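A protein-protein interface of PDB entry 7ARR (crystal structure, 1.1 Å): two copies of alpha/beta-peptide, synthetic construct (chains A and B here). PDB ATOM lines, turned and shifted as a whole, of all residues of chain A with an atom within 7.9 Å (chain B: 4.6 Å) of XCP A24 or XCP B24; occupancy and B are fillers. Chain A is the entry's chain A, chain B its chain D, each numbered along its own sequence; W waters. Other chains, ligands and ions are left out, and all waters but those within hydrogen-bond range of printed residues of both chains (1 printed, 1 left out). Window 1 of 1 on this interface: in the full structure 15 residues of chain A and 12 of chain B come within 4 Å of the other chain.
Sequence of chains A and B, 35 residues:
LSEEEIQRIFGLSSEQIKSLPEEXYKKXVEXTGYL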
ATOM      1  N   LEU A   1      21.637  29.714   7.041  1.00  0.00           N
ATOM      2  CA  LEU A   1      23.018  29.241   7.007  1.00  0.00           C
ATOM      3  C   LEU A   1      23.342  28.552   5.652  1.00  0.00           C
ATOM      4  O   LEU A   1      22.659  27.602   5.277  1.00  0.00           O
ATOM      5  CB  LEU A   1      23.140  28.394   8.279  1.00  0.00           C
ATOM      6  CG  LEU A   1      24.488  27.805   8.605  1.00  0.00           C
ATOM      7  CD1 LEU A   1      25.445  28.916   9.045  1.00  0.00           C
ATOM      8  CD2 LEU A   1      24.328  26.775   9.704  1.00  0.00           C
ATOM      9  N   ILE A   6      29.036  27.264   6.021  1.00  0.00           N
ATOM     10  CA  ILE A   6      29.475  26.039   6.733  1.00  0.00           C
ATOM     11  C   ILE A   6      30.915  25.657   6.350  1.00  0.00           C
ATOM     12  O   ILE A   6      31.697  25.312   7.244  1.00  0.00           O
ATOM     13  CB  ILE A   6      28.434  24.926   6.540  1.00  0.00           C
ATOM     14  CG1 ILE A   6      27.133  25.282   7.265  1.00  0.00           C
ATOM     15  CG2 ILE A   6      28.985  23.570   7.018  1.00  0.00           C
ATOM     16  CD1 ILE A   6      25.907  24.541   6.759  1.00  0.00           C
ATOM     17  N   GLN A   7      31.224  25.673   5.051  1.00  0.00           N
ATOM     18  CA  GLN A   7      32.593  25.342   4.628  1.00  0.00           C
ATOM     19  C   GLN A   7      33.596  26.225   5.357  1.00  0.00           C
ATOM     20  O   GLN A   7      34.623  25.703   5.846  1.00  0.00           O
ATOM     21  CB  GLN A   7      32.736  25.532   3.104  1.00  0.00           C
ATOM     22  CG  GLN A   7      34.100  25.226   2.471  1.00  0.00           C
ATOM     23  CD  GLN A   7      35.162  26.293   2.672  1.00  0.00           C
ATOM     24  OE1 GLN A   7      34.921  27.476   2.490  1.00  0.00           O
ATOM     25  NE2 GLN A   7      36.300  25.845   3.128  1.00  0.00           N
ATOM     26  N   ILE A   9      33.245  28.118   8.154  1.00  0.00           N
ATOM     27  CA  ILE A   9      33.221  28.024   9.611  1.00  0.00           C
ATOM     28  C   ILE A   9      33.987  26.809  10.073  1.00  0.00           C
ATOM     29  O   ILE A   9      34.652  26.867  11.108  1.00  0.00           O
ATOM     30  CB  ILE A   9      31.756  28.085  10.122  1.00  0.00           C
ATOM     31  CG1 ILE A   9      31.145  29.481   9.866  1.00  0.00           C
ATOM     32  CG2 ILE A   9      31.735  27.685  11.571  1.00  0.00           C
ATOM     33  CD1 ILE A   9      29.658  29.512  10.005  1.00  0.00           C
ATOM     34  N   PHE A  10      33.794  25.653   9.419  1.00  0.00           N
ATOM     35  CA  PHE A  10      34.387  24.381   9.854  1.00  0.00           C
ATOM     36  C   PHE A  10      35.636  24.038   9.048  1.00  0.00           C
ATOM     37  O   PHE A  10      36.107  22.928   9.208  1.00  0.00           O
ATOM     38  CB  PHE A  10      33.278  23.315   9.802  1.00  0.00           C
ATOM     39  CG  PHE A  10      32.164  23.576  10.795  1.00  0.00           C
ATOM     40  CD1 PHE A  10      32.334  23.374  12.147  1.00  0.00           C
ATOM     41  CD2 PHE A  10      30.988  24.164  10.389  1.00  0.00           C
ATOM     42  CE1 PHE A  10      31.336  23.656  13.053  1.00  0.00           C
ATOM     43  CE2 PHE A  10      29.969  24.452  11.294  1.00  0.00           C
ATOM     44  CZ  PHE A  10      30.180  24.227  12.636  1.00  0.00           C
ATOM     45  N   LEU A  12      36.226  23.276   5.988  1.00  0.00           N
ATOM     46  CA  LEU A  12      36.083  22.053   5.191  1.00  0.00           C
ATOM     47  C   LEU A  12      36.843  22.097   3.860  1.00  0.00           C
ATOM     48  O   LEU A  12      36.839  23.113   3.177  1.00  0.00           O
ATOM     49  CB  LEU A  12      34.627  21.746   4.950  1.00  0.00           C
ATOM     50  CG  LEU A  12      33.745  21.567   6.172  1.00  0.00           C
ATOM     51  CD1 LEU A  12      32.350  21.325   5.697  1.00  0.00           C
ATOM     52  CD2 LEU A  12      34.266  20.514   7.048  1.00  0.00           C
ATOM     53  N   GLN A  16      35.497  17.353   1.469  1.00  0.00           N
ATOM     54  CA  GLN A  16      34.589  17.257   2.607  1.00  0.00           C
ATOM     55  C   GLN A  16      33.245  17.888   2.289  1.00  0.00           C
ATOM     56  O   GLN A  16      32.206  17.451   2.805  1.00  0.00           O
ATOM     57  CB  GLN A  16      35.190  17.851   3.898  1.00  0.00           C
ATOM     58  CG  GLN A  16      36.280  16.968   4.464  1.00  0.00           C
ATOM     59  CD  GLN A  16      37.128  17.650   5.495  1.00  0.00           C
ATOM     60  OE1 GLN A  16      37.311  18.868   5.509  1.00  0.00           O
ATOM     61  NE2 GLN A  16      37.672  16.888   6.404  1.00  0.00           N
ATOM     62  N   ILE A  17      33.200  18.963   1.486  1.00  0.00           N
ATOM     63  CA  ILE A  17      31.936  19.659   1.200  1.00  0.00           C
ATOM     64  C   ILE A  17      31.001  18.796   0.317  1.00  0.00           C
ATOM     65  O   ILE A  17      29.834  19.112   0.244  1.00  0.00           O
ATOM     66  CB  ILE A  17      32.162  21.056   0.615  1.00  0.00           C
ATOM     67  CG1 ILE A  17      32.811  20.986  -0.754  1.00  0.00           C
ATOM     68  CG2 ILE A  17      32.936  21.972   1.566  1.00  0.00           C
ATOM     69  CD1 ILE A  17      32.873  22.292  -1.499  1.00  0.00           C
ATOM     70  N   SER A  19      30.117  15.968   1.271  1.00  0.00           N
ATOM     71  CA  SER A  19      29.415  15.189   2.312  1.00  0.00           C
ATOM     72  C   SER A  19      29.146  16.089   3.513  1.00  0.00           C
ATOM     73  O   SER A  19      29.620  15.828   4.594  1.00  0.00           O
ATOM     74  CB  SER A  19      30.168  13.955   2.712  1.00  0.00           C
ATOM     75  OG  SER A  19      30.426  13.130   1.574  1.00  0.00           O
ATOM     76  N   LEU A  20      28.412  17.181   3.303  1.00  0.00           N
ATOM     77  CA  LEU A  20      28.325  18.182   4.360  1.00  0.00           C
ATOM     78  C   LEU A  20      27.677  17.636   5.632  1.00  0.00           C
ATOM     79  O   LEU A  20      28.145  17.958   6.706  1.00  0.00           O
ATOM     80  CB  LEU A  20      27.531  19.421   3.922  1.00  0.00           C
ATOM     81  CG  LEU A  20      28.163  20.511   3.079  1.00  0.00           C
ATOM     82  CD1 LEU A  20      27.179  21.670   3.020  1.00  0.00           C
ATOM     83  CD2 LEU A  20      29.527  20.955   3.579  1.00  0.00           C
ATOM     84  N   PRO A  21      26.560  16.887   5.579  1.00  0.00           N
ATOM     85  CA  PRO A  21      25.963  16.403   6.845  1.00  0.00           C
ATOM     86  C   PRO A  21      26.922  15.561   7.660  1.00  0.00           C
ATOM     87  O   PRO A  21      27.010  15.689   8.874  1.00  0.00           O
ATOM     88  CB  PRO A  21      24.749  15.606   6.370  1.00  0.00           C
ATOM     89  CG  PRO A  21      24.385  16.260   5.053  1.00  0.00           C
ATOM     90  CD  PRO A  21      25.739  16.510   4.432  1.00  0.00           C
ATOM     91  N   GLU A  22      27.651  14.675   6.957  1.00  0.00           N
ATOM     92  CA  GLU A  22      28.560  13.756   7.657  1.00  0.00           C
ATOM     93  C   GLU A  22      29.775  14.501   8.180  1.00  0.00           C
ATOM     94  O   GLU A  22      30.277  14.256   9.261  1.00  0.00           O
ATOM     95  CB  GLU A  22      29.006  12.657   6.720  1.00  0.00           C
ATOM     96  CG  GLU A  22      27.884  11.783   6.152  1.00  0.00           C
ATOM     97  CD  GLU A  22      27.182  12.292   4.917  1.00  0.00           C
ATOM     98  OE1 GLU A  22      27.375  13.394   4.492  1.00  0.00           O
ATOM     99  OE2 GLU A  22      26.361  11.464   4.417  1.00  0.00           O
ATOM    100  N   GLU A  23      30.371  15.403   7.324  1.00  0.00           N
ATOM    101  CA  GLU A  23      31.689  16.024   7.709  1.00  0.00           C
ATOM    102  C   GLU A  23      31.431  17.177   8.675  1.00  0.00           C
ATOM    103  O   GLU A  23      32.334  17.366   9.543  1.00  0.00           O
ATOM    104  CB  GLU A  23      32.393  16.474   6.430  1.00  0.00           C
ATOM    105  CG  GLU A  23      32.773  15.287   5.578  1.00  0.00           C
ATOM    106  CD  GLU A  23      33.845  14.398   6.144  1.00  0.00           C
ATOM    107  OE1 GLU A  23      34.709  14.857   6.876  1.00  0.00           O
ATOM    108  OE2 GLU A  23      33.772  13.143   5.904  1.00  0.00           O
ATOM    109  N   XCP A  24      30.345  17.870   8.541  1.00  0.00           N
ATOM    110  CB  XCP A  24      29.985  18.940   9.482  1.00  0.00           C
ATOM    111  CG  XCP A  24      29.704  20.292   8.777  1.00  0.00           C
ATOM    112  CD  XCP A  24      28.978  21.107   9.853  1.00  0.00           C
ATOM    113  CE  XCP A  24      28.191  20.039  10.689  1.00  0.00           C
ATOM    114  CA  XCP A  24      28.640  18.672  10.207  1.00  0.00           C
ATOM    115  C   XCP A  24      28.919  17.722  11.400  1.00  0.00           C
ATOM    116  O   XCP A  24      29.389  18.095  12.441  1.00  0.00           O
ATOM    117  N   TYR A  25      28.501  16.434  11.202  1.00  0.00           N
ATOM    118  CA  TYR A  25      28.603  15.461  12.335  1.00  0.00           C
ATOM    119  C   TYR A  25      30.014  15.395  12.905  1.00  0.00           C
ATOM    120  O   TYR A  25      30.212  15.464  14.088  1.00  0.00           O
ATOM    121  CB  TYR A  25      28.132  14.098  11.780  1.00  0.00           C
ATOM    122  CG  TYR A  25      28.027  13.021  12.829  1.00  0.00           C
ATOM    123  CD1 TYR A  25      29.120  12.414  13.374  1.00  0.00           C
ATOM    124  CD2 TYR A  25      26.773  12.525  13.259  1.00  0.00           C
ATOM    125  CE1 TYR A  25      29.087  11.407  14.341  1.00  0.00           C
ATOM    126  CE2 TYR A  25      26.700  11.504  14.215  1.00  0.00           C
ATOM    127  CZ  TYR A  25      27.825  10.954  14.744  1.00  0.00           C
ATOM    128  OH  TYR A  25      27.760   9.977  15.711  1.00  0.00           O
ATOM    129  N   LYS A  26      31.025  15.237  11.991  1.00  0.00           N
ATOM    130  CA  LYS A  26      32.390  14.993  12.512  1.00  0.00           C
ATOM    131  C   LYS A  26      32.974  16.255  13.152  1.00  0.00           C
ATOM    132  O   LYS A  26      33.524  16.216  14.206  1.00  0.00           O
ATOM    133  CB  LYS A  26      33.293  14.501  11.403  1.00  0.00           C
ATOM    134  CG  LYS A  26      32.928  13.132  10.893  1.00  0.00           C
ATOM    135  CD  LYS A  26      33.804  12.713   9.729  1.00  0.00           C
ATOM    136  CE  LYS A  26      33.390  11.430   9.074  1.00  0.00           C
ATOM    137  NZ  LYS A  26      34.383  11.057   8.019  1.00  0.00           N
ATOM    138  N   LYS A  27      32.839  17.418  12.463  1.00  0.00           N
ATOM    139  CA  LYS A  27      33.466  18.664  12.988  1.00  0.00           C
ATOM    140  C   LYS A  27      32.750  19.170  14.220  1.00  0.00           C
ATOM    141  O   LYS A  27      33.334  19.790  15.094  1.00  0.00           O
ATOM    142  CB  LYS A  27      33.447  19.782  11.922  1.00  0.00           C
ATOM    143  CG  LYS A  27      34.455  19.541  10.832  1.00  0.00           C
ATOM    144  CD  LYS A  27      35.791  20.005  11.126  1.00  0.00           C
ATOM    145  CE  LYS A  27      36.717  19.849   9.967  1.00  0.00           C
ATOM    146  NZ  LYS A  27      37.838  20.760  10.000  1.00  0.00           N
ATOM    147  N   XCP A  28      31.400  18.889  14.299  1.00  0.00           N
ATOM    148  CB  XCP A  28      30.567  19.311  15.436  1.00  0.00           C
ATOM    149  CG  XCP A  28      29.550  20.350  15.137  1.00  0.00           C
ATOM    150  CD  XCP A  28      28.645  20.255  16.391  1.00  0.00           C
ATOM    151  CE  XCP A  28      28.500  18.811  16.602  1.00  0.00           C
ATOM    152  CA  XCP A  28      29.770  18.063  16.006  1.00  0.00           C
ATOM    153  C   XCP A  28      30.609  17.333  17.011  1.00  0.00           C
ATOM    154  O   XCP A  28      30.729  17.764  18.148  1.00  0.00           O
ATOM    155  N   VAL A  29      31.215  16.247  16.569  1.00  0.00           N
ATOM    156  CA  VAL A  29      32.027  15.482  17.505  1.00  0.00           C
ATOM    157  C   VAL A  29      33.208  16.288  18.027  1.00  0.00           C
ATOM    158  O   VAL A  29      33.475  16.318  19.212  1.00  0.00           O
ATOM    159  CB  VAL A  29      32.514  14.210  16.835  1.00  0.00           C
ATOM    160  CG1 VAL A  29      33.388  13.471  17.797  1.00  0.00           C
ATOM    161  CG2 VAL A  29      31.366  13.291  16.396  1.00  0.00           C
ATOM    162  N   GLU A  30      34.015  16.875  17.138  1.00  0.00           N
ATOM    163  CA  GLU A  30      35.236  17.625  17.568  1.00  0.00           C
ATOM    164  C   GLU A  30      34.819  18.847  18.402  1.00  0.00           C
ATOM    165  O   GLU A  30      35.357  18.950  19.550  1.00  0.00           O
ATOM    166  CB  GLU A  30      36.065  17.962  16.356  1.00  0.00           C
ATOM    167  CG  GLU A  30      37.340  18.692  16.697  1.00  0.00           C
ATOM    168  CD  GLU A  30      38.210  19.060  15.547  1.00  0.00           C
ATOM    169  OE1 GLU A  30      37.733  19.246  14.423  1.00  0.00           O
ATOM    170  OE2 GLU A  30      39.424  19.202  15.739  1.00  0.00           O
ATOM    171  N   XCP A  31      33.989  19.726  17.892  1.00  0.00           N
ATOM    172  CB  XCP A  31      33.504  20.862  18.692  1.00  0.00           C
ATOM    173  CG  XCP A  31      33.265  22.119  17.775  1.00  0.00           C
ATOM    174  CD  XCP A  31      31.825  22.555  17.983  1.00  0.00           C
ATOM    175  CE  XCP A  31      31.364  21.945  19.328  1.00  0.00           C
ATOM    176  CA  XCP A  31      32.087  20.586  19.302  1.00  0.00           C
ATOM    177  C   XCP A  31      32.217  19.947  20.650  1.00  0.00           C
ATOM    178  O   XCP A  31      32.601  20.574  21.662  1.00  0.00           O
ATOM    179  N   ILE B   6      27.339  26.573  18.938  1.00  0.00           N
ATOM    180  CA  ILE B   6      26.666  25.703  17.946  1.00  0.00           C
ATOM    181  C   ILE B   6      25.126  25.786  18.142  1.00  0.00           C
ATOM    182  O   ILE B   6      24.442  25.899  17.126  1.00  0.00           O
ATOM    183  CB  ILE B   6      27.110  24.241  18.085  1.00  0.00           C
ATOM    184  CG1 ILE B   6      28.589  24.133  17.714  1.00  0.00           C
ATOM    185  CG2 ILE B   6      26.242  23.280  17.297  1.00  0.00           C
ATOM    186  CD1 ILE B   6      28.912  24.326  16.242  1.00  0.00           C
ATOM    187  N   PHE B  10      22.862  27.256  14.950  1.00  0.00           N
ATOM    188  CA  PHE B  10      21.916  26.320  14.291  1.00  0.00           C
ATOM    189  C   PHE B  10      20.497  26.431  14.813  1.00  0.00           C
ATOM    190  O   PHE B  10      19.613  25.768  14.258  1.00  0.00           O
ATOM    191  CB  PHE B  10      22.407  24.876  14.373  1.00  0.00           C
ATOM    192  CG  PHE B  10      23.608  24.648  13.492  1.00  0.00           C
ATOM    193  CD1 PHE B  10      23.478  24.436  12.131  1.00  0.00           C
ATOM    194  CD2 PHE B  10      24.883  24.715  14.012  1.00  0.00           C
ATOM    195  CE1 PHE B  10      24.601  24.204  11.347  1.00  0.00           C
ATOM    196  CE2 PHE B  10      25.994  24.507  13.209  1.00  0.00           C
ATOM    197  CZ  PHE B  10      25.847  24.204  11.898  1.00  0.00           C
ATOM    198  N   LEU B  12      19.216  25.404  17.861  1.00  0.00           N
ATOM    199  CA  LEU B  12      18.862  24.091  18.416  1.00  0.00           C
ATOM    200  C   LEU B  12      18.077  24.262  19.676  1.00  0.00           C
ATOM    201  O   LEU B  12      18.455  25.063  20.569  1.00  0.00           O
ATOM    202  CB  LEU B  12      20.073  23.222  18.677  1.00  0.00           C
ATOM    203  CG  LEU B  12      21.017  22.879  17.547  1.00  0.00           C
ATOM    204  CD1 LEU B  12      22.232  22.133  18.083  1.00  0.00           C
ATOM    205  CD2 LEU B  12      20.314  22.079  16.514  1.00  0.00           C
ATOM    206  N   LEU B  20      24.403  16.362  19.982  1.00  0.00           N
ATOM    207  CA  LEU B  20      24.861  17.431  19.128  1.00  0.00           C
ATOM    208  C   LEU B  20      25.357  16.937  17.762  1.00  0.00           C
ATOM    209  O   LEU B  20      24.982  17.513  16.730  1.00  0.00           O
ATOM    210  CB  LEU B  20      25.921  18.285  19.821  1.00  0.00           C
ATOM    211  CG  LEU B  20      26.083  19.684  19.272  1.00  0.00           C
ATOM    212  CD1 LEU B  20      24.819  20.513  19.544  1.00  0.00           C
ATOM    213  CD2 LEU B  20      27.268  20.376  19.929  1.00  0.00           C
ATOM    214  N   PRO B  21      26.197  15.898  17.653  1.00  0.00           N
ATOM    215  CA  PRO B  21      26.650  15.422  16.335  1.00  0.00           C
ATOM    216  C   PRO B  21      25.495  15.091  15.399  1.00  0.00           C
ATOM    217  O   PRO B  21      25.450  15.389  14.211  1.00  0.00           O
ATOM    218  CB  PRO B  21      27.559  14.269  16.641  1.00  0.00           C
ATOM    219  CG  PRO B  21      28.064  14.590  18.022  1.00  0.00           C
ATOM    220  CD  PRO B  21      26.880  15.185  18.721  1.00  0.00           C
ATOM    221  N   GLU B  22      24.527  14.336  15.990  1.00  0.00           N
ATOM    222  CA  GLU B  22      23.345  13.893  15.159  1.00  0.00           C
ATOM    223  C   GLU B  22      22.418  15.100  14.816  1.00  0.00           C
ATOM    224  O   GLU B  22      21.990  15.205  13.694  1.00  0.00           O
ATOM    225  CB  GLU B  22      22.518  12.853  15.938  1.00  0.00           C
ATOM    226  CG  GLU B  22      23.318  11.509  16.096  1.00  0.00           C
ATOM    227  CD  GLU B  22      22.603  10.405  16.842  1.00  0.00           C
ATOM    228  OE1 GLU B  22      21.441  10.692  17.322  1.00  0.00           O
ATOM    229  OE2 GLU B  22      23.176   9.317  17.040  1.00  0.00           O
ATOM    230  N   GLU B  23      22.070  15.904  15.796  1.00  0.00           N
ATOM    231  CA  GLU B  23      21.082  16.977  15.553  1.00  0.00           C
ATOM    232  C   GLU B  23      21.616  18.109  14.707  1.00  0.00           C
ATOM    233  O   GLU B  23      20.936  18.694  13.891  1.00  0.00           O
ATOM    234  CB  GLU B  23      20.524  17.446  16.862  1.00  0.00           C
ATOM    235  CG  GLU B  23      19.696  16.376  17.558  1.00  0.00           C
ATOM    236  CD  GLU B  23      18.417  15.926  16.803  1.00  0.00           C
ATOM    237  OE1 GLU B  23      17.759  16.789  16.174  1.00  0.00           O
ATOM    238  OE2 GLU B  23      18.113  14.678  16.762  1.00  0.00           O
ATOM    239  N   XCP B  24      22.947  18.375  14.917  1.00  0.00           N
ATOM    240  CB  XCP B  24      23.700  19.395  14.162  1.00  0.00           C
ATOM    241  CG  XCP B  24      24.263  20.511  15.020  1.00  0.00           C
ATOM    242  CD  XCP B  24      25.512  20.943  14.364  1.00  0.00           C
ATOM    243  CE  XCP B  24      25.844  19.959  13.274  1.00  0.00           C
ATOM    244  CA  XCP B  24      24.854  18.793  13.406  1.00  0.00           C
ATOM    245  C   XCP B  24      24.419  18.241  12.045  1.00  0.00           C
ATOM    246  O   XCP B  24      24.067  18.963  11.141  1.00  0.00           O
ATOM    247  N   TYR B  25      24.422  16.839  12.006  1.00  0.00           N
ATOM    248  CA  TYR B  25      24.041  16.230  10.740  1.00  0.00           C
ATOM    249  C   TYR B  25      22.716  16.730  10.208  1.00  0.00           C
ATOM    250  O   TYR B  25      22.541  17.025   9.020  1.00  0.00           O
ATOM    251  CB  TYR B  25      23.972  14.706  10.969  1.00  0.00           C
ATOM    252  CG  TYR B  25      23.688  13.881   9.771  1.00  0.00           C
ATOM    253  CD1 TYR B  25      22.357  13.686   9.379  1.00  0.00           C
ATOM    254  CD2 TYR B  25      24.677  13.189   9.115  1.00  0.00           C
ATOM    255  CE1 TYR B  25      22.075  12.933   8.258  1.00  0.00           C
ATOM    256  CE2 TYR B  25      24.344  12.428   7.999  1.00  0.00           C
ATOM    257  CZ  TYR B  25      23.053  12.278   7.573  1.00  0.00           C
ATOM    258  OH  TYR B  25      22.771  11.543   6.429  1.00  0.00           O
ATOM    259  N   LYS B  26      21.670  16.684  11.075  1.00  0.00           N
ATOM    260  CA  LYS B  26      20.302  17.020  10.577  1.00  0.00           C
ATOM    261  C   LYS B  26      20.147  18.474  10.197  1.00  0.00           C
ATOM    262  O   LYS B  26      19.580  18.756   9.124  1.00  0.00           O
ATOM    263  CB  LYS B  26      19.276  16.596  11.593  1.00  0.00           C
ATOM    264  CG  LYS B  26      19.189  15.067  11.741  1.00  0.00           C
ATOM    265  CD  LYS B  26      18.327  14.555  12.908  1.00  0.00           C
ATOM    266  CE  LYS B  26      17.049  15.221  13.094  1.00  0.00           C
ATOM    267  NZ  LYS B  26      16.303  14.592  14.180  1.00  0.00           N
ATOM    268  N   LYS B  27      20.600  19.431  11.023  1.00  0.00           N
ATOM    269  CA  LYS B  27      20.444  20.837  10.643  1.00  0.00           C
ATOM    270  C   LYS B  27      21.368  21.203   9.512  1.00  0.00           C
ATOM    271  O   LYS B  27      20.968  22.087   8.758  1.00  0.00           O
ATOM    272  CB  LYS B  27      20.766  21.763  11.821  1.00  0.00           C
ATOM    273  CG  LYS B  27      19.777  21.746  12.948  1.00  0.00           C
ATOM    274  CD  LYS B  27      18.432  22.274  12.574  1.00  0.00           C
ATOM    275  CE  LYS B  27      17.543  22.334  13.803  1.00  0.00           C
ATOM    276  NZ  LYS B  27      16.423  23.258  13.524  1.00  0.00           N
ATOM    277  N   XCP B  28      22.523  20.605   9.418  1.00  0.00           N
ATOM    278  CB  XCP B  28      23.454  20.949   8.308  1.00  0.00           C
ATOM    279  CG  XCP B  28      24.862  21.313   8.825  1.00  0.00           C
ATOM    280  CD  XCP B  28      25.788  20.634   7.836  1.00  0.00           C
ATOM    281  CE  XCP B  28      25.042  20.027   6.795  1.00  0.00           C
ATOM    282  CA  XCP B  28      23.759  19.682   7.479  1.00  0.00           C
ATOM    283  C   XCP B  28      22.692  19.429   6.455  1.00  0.00           C
ATOM    284  O   XCP B  28      22.591  20.152   5.426  1.00  0.00           O
HETATM  285  O   HOH W   1      25.542   8.607  15.995  1.00  0.00           O
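NZ of Lys A27 sits at hydrogen-bond distance from O of Phe A10 (2.9 Å).
Among the printed residues, merely in contact across the chains: Leu A1 with Phe B10 (3.1 Å), Ile A6 with XCP B28 (3.97 Å), Phe A10 with Ile B6 (3.8 Å), Leu A20 with XCP B28 (3.7 Å), Pro A21 with Tyr B25 (3.4 Å), Pro A21 with XCP B28 (3.7 Å), Glu A22 with Tyr B25 (3.96 Å), XCP A24 with XCP B24 (3.5 Å), XCP A24 with XCP B28 (3.8 Å), Tyr A25 with Pro B21 (3.3 Å), Tyr A25 with Glu B22 (3.9 Å), XCP A28 with Ile B6 (3.97 Å), XCP A28 with Leu B20 (3.7 Å), XCP A28 with Pro B21 (3.9 Å), XCP A28 with XCP B24 (3.8 Å), Val A29 with Pro B21 (3.8 Å) and XCP A31 with Ile B6 (3.6 Å).
Printed residues of chain B within 4 Å of Tyr A25: Pro B21 (3.3 Å) and Glu B22 (3.9 Å).
Of the printed residues of chain B, XCP A31 touches Ile B6.
Of the printed residues of chain A, Ile B6 touches Phe A10, XCP A28 and XCP A31.
Of the printed residues of chain A, Phe B10 touches Leu A1.
Of chain A, only XCP A24 and XCP A28 come within 4 Å of XCP B24.
The nearest printed residue of chain B that does not touch XCP A24 is Tyr B25 (4.6 Å).
Of the 21 printed residues of chain A, 11 touch a printed residue of chain B.
Printed residues of chain A that touch a printed residue of chain B: Leu A1, Ile A6, Phe A10, Leu A20, Pro A21, Glu A22, XCP A24, Tyr A25, XCP A28, Val A29 and XCP A31.
Of the 12 printed residues of chain B, 8 touch a printed residue of chain A.
Among the printed residues, 17 pairs touch across the chains.
Among the printed residues, no Asp or Glu carboxylate lies within 4 Å of a Lys or Arg side-chain nitrogen of the other chain.
Phe A10 touches Ile B6, but with the chains exchanged Ile A6 does not touch Phe B10 (4.8 Å).
Leu A20 touches XCP B28, and with the chains exchanged XCP A28 touches Leu B20.
Pro A21 touches Tyr B25, and with the chains exchanged Tyr A25 touches Pro B21.
Glu A22 touches Tyr B25, and with the chains exchanged Tyr A25 touches Glu B22.
12 positions are printed for both chains.
Of the 17 pairs that touch across the chains among the printed residues, 13 have their exchanged pair printed and touching as well.
Water W1 lies within hydrogen-bond range of the side-chain hydroxyl of Tyr A25 (2.6 Å) and the side-chain carboxylate of Glu B22 (2.7 Å).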
